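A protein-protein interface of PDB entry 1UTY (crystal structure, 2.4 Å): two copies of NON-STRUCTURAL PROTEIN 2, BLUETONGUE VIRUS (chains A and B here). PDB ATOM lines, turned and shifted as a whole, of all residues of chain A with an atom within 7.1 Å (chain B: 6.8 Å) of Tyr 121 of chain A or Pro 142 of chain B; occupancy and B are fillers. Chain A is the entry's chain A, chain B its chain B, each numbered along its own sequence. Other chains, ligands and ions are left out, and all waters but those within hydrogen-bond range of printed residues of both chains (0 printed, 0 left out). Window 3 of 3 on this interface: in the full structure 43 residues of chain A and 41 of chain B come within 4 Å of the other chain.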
ATOM      1  N   LEU A  15      14.017 -18.095 -15.414  1.00  0.00           N
ATOM      2  CA  LEU A  15      13.719 -19.508 -15.353  1.00  0.00           C
ATOM      3  C   LEU A  15      13.930 -20.024 -16.768  1.00  0.00           C
ATOM      4  O   LEU A  15      13.157 -19.697 -17.686  1.00  0.00           O
ATOM      5  CB  LEU A  15      12.279 -19.735 -14.885  1.00  0.00           C
ATOM      6  CG  LEU A  15      11.749 -21.182 -14.936  1.00  0.00           C
ATOM      7  CD1 LEU A  15      12.560 -22.122 -14.029  1.00  0.00           C
ATOM      8  CD2 LEU A  15      10.243 -21.254 -14.588  1.00  0.00           C
ATOM      9  N   GLY A  55       9.858  -8.936  -7.480  1.00  0.00           N
ATOM     10  CA  GLY A  55      10.679  -9.462  -8.558  1.00  0.00           C
ATOM     11  C   GLY A  55       9.919  -9.939  -9.794  1.00  0.00           C
ATOM     12  O   GLY A  55       8.697 -10.195  -9.751  1.00  0.00           O
ATOM     13  N   TYR A  56      10.658 -10.064 -10.890  1.00  0.00           N
ATOM     14  CA  TYR A  56      10.130 -10.551 -12.165  1.00  0.00           C
ATOM     15  C   TYR A  56      10.613 -11.973 -12.380  1.00  0.00           C
ATOM     16  O   TYR A  56      11.814 -12.237 -12.278  1.00  0.00           O
ATOM     17  CB  TYR A  56      10.622  -9.678 -13.339  1.00  0.00           C
ATOM     18  CG  TYR A  56      10.182  -8.237 -13.254  1.00  0.00           C
ATOM     19  CD1 TYR A  56      10.804  -7.341 -12.378  1.00  0.00           C
ATOM     20  CD2 TYR A  56       9.129  -7.772 -14.030  1.00  0.00           C
ATOM     21  CE1 TYR A  56      10.373  -6.013 -12.282  1.00  0.00           C
ATOM     22  CE2 TYR A  56       8.703  -6.460 -13.945  1.00  0.00           C
ATOM     23  CZ  TYR A  56       9.329  -5.591 -13.078  1.00  0.00           C
ATOM     24  OH  TYR A  56       8.900  -4.299 -13.023  1.00  0.00           O
ATOM     25  N   VAL A  57       9.692 -12.886 -12.656  1.00  0.00           N
ATOM     26  CA  VAL A  57      10.083 -14.202 -13.121  1.00  0.00           C
ATOM     27  C   VAL A  57      10.002 -14.159 -14.638  1.00  0.00           C
ATOM     28  O   VAL A  57       8.941 -13.946 -15.220  1.00  0.00           O
ATOM     29  CB  VAL A  57       9.197 -15.334 -12.552  1.00  0.00           C
ATOM     30  CG1 VAL A  57       9.497 -16.656 -13.233  1.00  0.00           C
ATOM     31  CG2 VAL A  57       9.384 -15.458 -11.049  1.00  0.00           C
ATOM     32  N   LEU A  58      11.153 -14.318 -15.266  1.00  0.00           N
ATOM     33  CA  LEU A  58      11.237 -14.374 -16.698  1.00  0.00           C
ATOM     34  C   LEU A  58      11.442 -15.833 -17.098  1.00  0.00           C
ATOM     35  O   LEU A  58      12.558 -16.362 -17.065  1.00  0.00           O
ATOM     36  CB  LEU A  58      12.378 -13.483 -17.187  1.00  0.00           C
ATOM     37  CG  LEU A  58      12.581 -13.389 -18.704  1.00  0.00           C
ATOM     38  CD1 LEU A  58      11.246 -13.049 -19.418  1.00  0.00           C
ATOM     39  CD2 LEU A  58      13.695 -12.377 -19.027  1.00  0.00           C
ATOM     40  N   ASN A  59      10.330 -16.477 -17.427  1.00  0.00           N
ATOM     41  CA  ASN A  59      10.304 -17.841 -17.922  1.00  0.00           C
ATOM     42  C   ASN A  59      10.597 -17.762 -19.419  1.00  0.00           C
ATOM     43  O   ASN A  59       9.808 -17.181 -20.186  1.00  0.00           O
ATOM     44  CB  ASN A  59       8.919 -18.418 -17.634  1.00  0.00           C
ATOM     45  CG  ASN A  59       8.744 -19.884 -18.080  1.00  0.00           C
ATOM     46  OD1 ASN A  59       9.566 -20.447 -18.777  1.00  0.00           O
ATOM     47  ND2 ASN A  59       7.624 -20.476 -17.692  1.00  0.00           N
ATOM     48  N   VAL A  60      11.753 -18.280 -19.839  1.00  0.00           N
ATOM     49  CA  VAL A  60      12.067 -18.344 -21.275  1.00  0.00           C
ATOM     50  C   VAL A  60      12.365 -19.769 -21.730  1.00  0.00           C
ATOM     51  O   VAL A  60      12.742 -20.595 -20.911  1.00  0.00           O
ATOM     52  CB  VAL A  60      13.219 -17.363 -21.708  1.00  0.00           C
ATOM     53  CG1 VAL A  60      12.921 -15.941 -21.264  1.00  0.00           C
ATOM     54  CG2 VAL A  60      14.568 -17.815 -21.214  1.00  0.00           C
ATOM     55  N   VAL A  99       7.453  -8.788 -23.767  1.00  0.00           N
ATOM     56  CA  VAL A  99       6.939  -9.761 -22.827  1.00  0.00           C
ATOM     57  C   VAL A  99       6.035  -8.996 -21.873  1.00  0.00           C
ATOM     58  O   VAL A  99       6.409  -7.918 -21.374  1.00  0.00           O
ATOM     59  CB  VAL A  99       8.098 -10.440 -22.051  1.00  0.00           C
ATOM     60  CG1 VAL A  99       7.570 -11.416 -21.015  1.00  0.00           C
ATOM     61  CG2 VAL A  99       9.059 -11.141 -23.019  1.00  0.00           C
ATOM     62  N   SER A 100       4.847  -9.544 -21.646  1.00  0.00           N
ATOM     63  CA  SER A 100       3.897  -8.991 -20.691  1.00  0.00           C
ATOM     64  C   SER A 100       4.124  -9.462 -19.239  1.00  0.00           C
ATOM     65  O   SER A 100       4.663 -10.551 -18.976  1.00  0.00           O
ATOM     66  CB  SER A 100       2.466  -9.348 -21.111  1.00  0.00           C
ATOM     67  OG  SER A 100       2.035  -8.545 -22.198  1.00  0.00           O
ATOM     68  N   VAL A 101       3.661  -8.638 -18.309  1.00  0.00           N
ATOM     69  CA  VAL A 101       3.730  -8.938 -16.900  1.00  0.00           C
ATOM     70  C   VAL A 101       2.340  -9.327 -16.431  1.00  0.00           C
ATOM     71  O   VAL A 101       1.369  -8.641 -16.721  1.00  0.00           O
ATOM     72  CB  VAL A 101       4.190  -7.687 -16.109  1.00  0.00           C
ATOM     73  CG1 VAL A 101       3.900  -7.837 -14.632  1.00  0.00           C
ATOM     74  CG2 VAL A 101       5.648  -7.442 -16.335  1.00  0.00           C
ATOM     75  N   THR A 102       2.252 -10.434 -15.703  1.00  0.00           N
ATOM     76  CA  THR A 102       1.030 -10.779 -14.990  1.00  0.00           C
ATOM     77  C   THR A 102       1.410 -10.908 -13.525  1.00  0.00           C
ATOM     78  O   THR A 102       2.150 -11.803 -13.171  1.00  0.00           O
ATOM     79  CB  THR A 102       0.422 -12.102 -15.512  1.00  0.00           C
ATOM     80  OG1 THR A 102       0.286 -12.052 -16.939  1.00  0.00           O
ATOM     81  CG2 THR A 102      -1.011 -12.254 -15.017  1.00  0.00           C
ATOM     82  N   PRO A 103       0.950  -9.990 -12.687  1.00  0.00           N
ATOM     83  CA  PRO A 103       1.258 -10.047 -11.256  1.00  0.00           C
ATOM     84  C   PRO A 103       0.710 -11.317 -10.595  1.00  0.00           C
ATOM     85  O   PRO A 103      -0.306 -11.854 -11.019  1.00  0.00           O
ATOM     86  CB  PRO A 103       0.570  -8.794 -10.697  1.00  0.00           C
ATOM     87  CG  PRO A 103      -0.426  -8.389 -11.725  1.00  0.00           C
ATOM     88  CD  PRO A 103       0.135  -8.812 -13.042  1.00  0.00           C
ATOM     89  N   MET A 104       1.402 -11.802  -9.575  1.00  0.00           N
ATOM     90  CA  MET A 104       0.984 -13.000  -8.859  1.00  0.00           C
ATOM     91  C   MET A 104       1.058 -12.717  -7.387  1.00  0.00           C
ATOM     92  O   MET A 104       2.053 -12.173  -6.910  1.00  0.00           O
ATOM     93  CB  MET A 104       1.918 -14.180  -9.155  1.00  0.00           C
ATOM     94  CG  MET A 104       1.892 -14.667 -10.586  1.00  0.00           C
ATOM     95  SD  MET A 104       2.822 -16.181 -10.801  1.00  0.00           S
ATOM     96  CE  MET A 104       4.483 -15.676 -10.239  1.00  0.00           C
ATOM     97  N   ILE A 119       4.837 -11.055  -7.059  1.00  0.00           N
ATOM     98  CA  ILE A 119       5.829 -11.408  -8.060  1.00  0.00           C
ATOM     99  C   ILE A 119       5.234 -11.119  -9.425  1.00  0.00           C
ATOM    100  O   ILE A 119       4.049 -11.308  -9.643  1.00  0.00           O
ATOM    101  CB  ILE A 119       6.222 -12.891  -7.961  1.00  0.00           C
ATOM    102  CG1 ILE A 119       6.503 -13.293  -6.509  1.00  0.00           C
ATOM    103  CG2 ILE A 119       7.440 -13.190  -8.832  1.00  0.00           C
ATOM    104  CD1 ILE A 119       7.889 -12.975  -5.994  1.00  0.00           C
ATOM    105  N   LYS A 120       6.060 -10.666 -10.354  1.00  0.00           N
ATOM    106  CA  LYS A 120       5.568 -10.377 -11.686  1.00  0.00           C
ATOM    107  C   LYS A 120       5.982 -11.508 -12.605  1.00  0.00           C
ATOM    108  O   LYS A 120       7.180 -11.725 -12.821  1.00  0.00           O
ATOM    109  CB  LYS A 120       6.066  -9.005 -12.163  1.00  0.00           C
ATOM    110  CG  LYS A 120       6.091  -7.985 -11.037  1.00  0.00           C
ATOM    111  CD  LYS A 120       5.666  -6.606 -11.454  1.00  0.00           C
ATOM    112  CE  LYS A 120       6.358  -5.582 -10.556  1.00  0.00           C
ATOM    113  NZ  LYS A 120       5.675  -4.260 -10.621  1.00  0.00           N
ATOM    114  N   TYR A 121       4.990 -12.258 -13.093  1.00  0.00           N
ATOM    115  CA  TYR A 121       5.240 -13.388 -13.986  1.00  0.00           C
ATOM    116  C   TYR A 121       5.282 -12.973 -15.459  1.00  0.00           C
ATOM    117  O   TYR A 121       4.352 -12.330 -15.966  1.00  0.00           O
ATOM    118  CB  TYR A 121       4.214 -14.512 -13.788  1.00  0.00           C
ATOM    119  CG  TYR A 121       4.536 -15.728 -14.632  1.00  0.00           C
ATOM    120  CD1 TYR A 121       5.672 -16.510 -14.368  1.00  0.00           C
ATOM    121  CD2 TYR A 121       3.750 -16.067 -15.722  1.00  0.00           C
ATOM    122  CE1 TYR A 121       5.989 -17.609 -15.160  1.00  0.00           C
ATOM    123  CE2 TYR A 121       4.058 -17.165 -16.518  1.00  0.00           C
ATOM    124  CZ  TYR A 121       5.172 -17.932 -16.232  1.00  0.00           C
ATOM    125  OH  TYR A 121       5.474 -19.018 -17.030  1.00  0.00           O
ATOM    126  N   CYS A 122       6.351 -13.373 -16.141  1.00  0.00           N
ATOM    127  CA  CYS A 122       6.613 -12.963 -17.519  1.00  0.00           C
ATOM    128  C   CYS A 122       7.032 -14.179 -18.325  1.00  0.00           C
ATOM    129  O   CYS A 122       8.024 -14.843 -17.990  1.00  0.00           O
ATOM    130  CB  CYS A 122       7.728 -11.920 -17.575  1.00  0.00           C
ATOM    131  SG  CYS A 122       7.558 -10.571 -16.403  1.00  0.00           S
ATOM    132  N   LYS A 123       6.266 -14.479 -19.368  1.00  0.00           N
ATOM    133  CA  LYS A 123       6.547 -15.624 -20.207  1.00  0.00           C
ATOM    134  C   LYS A 123       6.939 -15.155 -21.599  1.00  0.00           C
ATOM    135  O   LYS A 123       6.160 -14.496 -22.291  1.00  0.00           O
ATOM    136  CB  LYS A 123       5.349 -16.603 -20.256  1.00  0.00           C
ATOM    137  CG  LYS A 123       5.582 -17.821 -21.171  1.00  0.00           C
ATOM    138  CD  LYS A 123       4.868 -19.076 -20.686  1.00  0.00           C
ATOM    139  CE  LYS A 123       5.004 -20.254 -21.680  1.00  0.00           C
ATOM    140  NZ  LYS A 123       6.409 -20.446 -22.216  1.00  0.00           N
ATOM    141  N   GLY A 124       8.158 -15.489 -21.994  1.00  0.00           N
ATOM    142  CA  GLY A 124       8.673 -15.147 -23.307  1.00  0.00           C
ATOM    143  C   GLY A 124       8.657 -16.392 -24.166  1.00  0.00           C
ATOM    144  O   GLY A 124       8.811 -17.491 -23.660  1.00  0.00           O
ATOM    145  N   PHE B 136      -4.325 -14.343 -12.790  1.00  0.00           N
ATOM    146  CA  PHE B 136      -4.412 -15.791 -12.863  1.00  0.00           C
ATOM    147  C   PHE B 136      -5.567 -16.325 -12.037  1.00  0.00           C
ATOM    148  O   PHE B 136      -5.620 -16.108 -10.826  1.00  0.00           O
ATOM    149  CB  PHE B 136      -3.099 -16.430 -12.418  1.00  0.00           C
ATOM    150  CG  PHE B 136      -1.970 -16.240 -13.393  1.00  0.00           C
ATOM    151  CD1 PHE B 136      -2.083 -16.690 -14.710  1.00  0.00           C
ATOM    152  CD2 PHE B 136      -0.795 -15.613 -12.994  1.00  0.00           C
ATOM    153  CE1 PHE B 136      -1.050 -16.512 -15.615  1.00  0.00           C
ATOM    154  CE2 PHE B 136       0.254 -15.439 -13.883  1.00  0.00           C
ATOM    155  CZ  PHE B 136       0.130 -15.886 -15.201  1.00  0.00           C
ATOM    156  N   ASP B 137      -6.499 -17.004 -12.705  1.00  0.00           N
ATOM    157  CA  ASP B 137      -7.535 -17.771 -12.015  1.00  0.00           C
ATOM    158  C   ASP B 137      -6.875 -18.928 -11.262  1.00  0.00           C
ATOM    159  O   ASP B 137      -5.755 -19.334 -11.598  1.00  0.00           O
ATOM    160  CB  ASP B 137      -8.587 -18.285 -13.001  1.00  0.00           C
ATOM    161  CG  ASP B 137     -10.007 -17.890 -12.598  1.00  0.00           C
ATOM    162  OD1 ASP B 137     -10.675 -18.682 -11.892  1.00  0.00           O
ATOM    163  OD2 ASP B 137     -10.532 -16.804 -12.944  1.00  0.00           O
ATOM    164  N   ASN B 139      -6.967 -21.894 -11.394  1.00  0.00           N
ATOM    165  CA  ASN B 139      -6.588 -23.015 -12.257  1.00  0.00           C
ATOM    166  C   ASN B 139      -5.299 -22.742 -13.042  1.00  0.00           C
ATOM    167  O   ASN B 139      -4.371 -23.548 -13.023  1.00  0.00           O
ATOM    168  CB  ASN B 139      -7.743 -23.361 -13.216  1.00  0.00           C
ATOM    169  N   GLU B 140      -5.248 -21.598 -13.722  1.00  0.00           N
ATOM    170  CA  GLU B 140      -4.142 -21.279 -14.632  1.00  0.00           C
ATOM    171  C   GLU B 140      -2.879 -20.714 -13.953  1.00  0.00           C
ATOM    172  O   GLU B 140      -1.955 -20.257 -14.635  1.00  0.00           O
ATOM    173  CB  GLU B 140      -4.624 -20.348 -15.746  1.00  0.00           C
ATOM    174  CG  GLU B 140      -5.896 -19.583 -15.408  1.00  0.00           C
ATOM    175  CD  GLU B 140      -5.956 -18.226 -16.085  1.00  0.00           C
ATOM    176  OE1 GLU B 140      -5.224 -18.017 -17.079  1.00  0.00           O
ATOM    177  OE2 GLU B 140      -6.732 -17.364 -15.623  1.00  0.00           O
ATOM    178  N   MET B 141      -2.847 -20.772 -12.623  1.00  0.00           N
ATOM    179  CA  MET B 141      -1.718 -20.293 -11.831  1.00  0.00           C
ATOM    180  C   MET B 141      -0.471 -21.168 -12.084  1.00  0.00           C
ATOM    181  O   MET B 141      -0.492 -22.374 -11.818  1.00  0.00           O
ATOM    182  CB  MET B 141      -2.095 -20.267 -10.339  1.00  0.00           C
ATOM    183  CG  MET B 141      -1.133 -19.472  -9.450  1.00  0.00           C
ATOM    184  SD  MET B 141      -1.634 -17.742  -9.061  1.00  0.00           S
ATOM    185  CE  MET B 141      -0.303 -17.341  -7.809  1.00  0.00           C
ATOM    186  N   PRO B 142       0.597 -20.559 -12.610  1.00  0.00           N
ATOM    187  CA  PRO B 142       1.805 -21.300 -12.992  1.00  0.00           C
ATOM    188  C   PRO B 142       2.514 -21.848 -11.771  1.00  0.00           C
ATOM    189  O   PRO B 142       2.539 -21.194 -10.725  1.00  0.00           O
ATOM    190  CB  PRO B 142       2.687 -20.241 -13.668  1.00  0.00           C
ATOM    191  CG  PRO B 142       1.805 -19.075 -13.907  1.00  0.00           C
ATOM    192  CD  PRO B 142       0.734 -19.114 -12.864  1.00  0.00           C
ATOM    193  N   ASP B 143       3.066 -23.047 -11.906  1.00  0.00           N
ATOM    194  CA  ASP B 143       3.803 -23.650 -10.814  1.00  0.00           C
ATOM    195  C   ASP B 143       5.247 -23.263 -10.976  1.00  0.00           C
ATOM    196  O   ASP B 143       5.850 -23.481 -12.026  1.00  0.00           O
ATOM    197  CB  ASP B 143       3.623 -25.165 -10.783  1.00  0.00           C
ATOM    198  CG  ASP B 143       2.205 -25.557 -10.483  1.00  0.00           C
ATOM    199  OD1 ASP B 143       1.431 -25.748 -11.436  1.00  0.00           O
ATOM    200  OD2 ASP B 143       1.764 -25.668  -9.326  1.00  0.00           O
ATOM    201  N   LEU B 144       5.778 -22.646  -9.936  1.00  0.00           N
ATOM    202  CA  LEU B 144       7.124 -22.116  -9.985  1.00  0.00           C
ATOM    203  C   LEU B 144       7.880 -22.543  -8.750  1.00  0.00           C
ATOM    204  O   LEU B 144       7.371 -22.427  -7.631  1.00  0.00           O
ATOM    205  CB  LEU B 144       7.102 -20.587 -10.133  1.00  0.00           C
ATOM    206  CG  LEU B 144       6.403 -20.019 -11.373  1.00  0.00           C
ATOM    207  CD1 LEU B 144       6.249 -18.519 -11.266  1.00  0.00           C
ATOM    208  CD2 LEU B 144       7.152 -20.386 -12.643  1.00  0.00           C
ATOM    209  N   VAL B 147       7.988 -20.889  -5.205  1.00  0.00           N
ATOM    210  CA  VAL B 147       6.849 -19.979  -5.149  1.00  0.00           C
ATOM    211  C   VAL B 147       5.628 -20.683  -4.548  1.00  0.00           C
ATOM    212  O   VAL B 147       5.030 -21.556  -5.179  1.00  0.00           O
ATOM    213  CB  VAL B 147       6.529 -19.373  -6.539  1.00  0.00           C
ATOM    214  CG1 VAL B 147       5.349 -18.447  -6.459  1.00  0.00           C
ATOM    215  CG2 VAL B 147       7.731 -18.621  -7.087  1.00  0.00           C
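Of the 19 printed residues of chain A, 4 touch a printed residue of chain B. Hydrophobic or aromatic side chains of chain A that line the printed part of chain B: Leu 15, Met 104 and Tyr 121. Of the 9 printed residues of chain B, 3 touch a printed residue of chain A.
The backbone carbonyl oxygen (O) of Leu 58 of chain A is in hydrogen-bond range of the backbone NH (N) of Leu 15 of chain A (2.8 Å). The backbone carbonyl oxygen (O) of Leu 15 of chain A lies within hydrogen-bond range of the backbone NH (N) of Val 60 of chain A (2.9 Å). ND2 of Asn 59 of chain A sits at hydrogen-bond distance from OH of Tyr 121 of chain A. N of Thr 102 of chain A is in hydrogen-bond range of O of Tyr 121 of chain A. The backbone carbonyl oxygen (O) of Ile 119 of chain A is in hydrogen-bond range of the backbone NH (N) of Met 104 of chain A (2.7 Å).
Of the printed residues of chain B, Leu 15 of chain A touches Leu 144 (3.8 Å). Of the printed residues of chain B, Thr 102 of chain A touches Phe 136. Printed residues of chain B within 4 Å of Met 104 of chain A: Phe 136 and Leu 144. Of chain B, only Phe 136, Pro 142 and Leu 144 come within 4 Å of Tyr 121 of chain A. Of the printed residues of chain A, Phe 136 of chain B touches Thr 102, Met 104 and Tyr 121. Pro 142 of chain B touches just one residue of chain A: Tyr 121. Printed residues of chain A within 4 Å of Leu 144 of chain B: Leu 15 (3.8 Å), Met 104 (3.5 Å) and Tyr 121 (3.7 Å). The nearest residue of chain B that does not touch Tyr 121 of chain A is Asp 143 of chain B (6.7 Å). The nearest printed residue of chain A that does not touch Phe 136 of chain B is Pro 103 of chain A (4.3 Å).
Among the printed residues, merely in contact across the chains: Leu 15 of chain A with Leu 144 of chain B, Thr 102 of chain A with Phe 136 of chain B, Met 104 of chain A with Phe 136 of chain B, Met 104 of chain A with Leu 144 of chain B, Tyr 121 of chain A with Phe 136 of chain B, Tyr 121 of chain A with Pro 142 of chain B and Tyr 121 of chain A with Leu 144 of chain B.
No position is printed for both chains. Of the 7 pairs that touch across the chains among the printed residues, none has its exchanged pair printed and touching as well.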
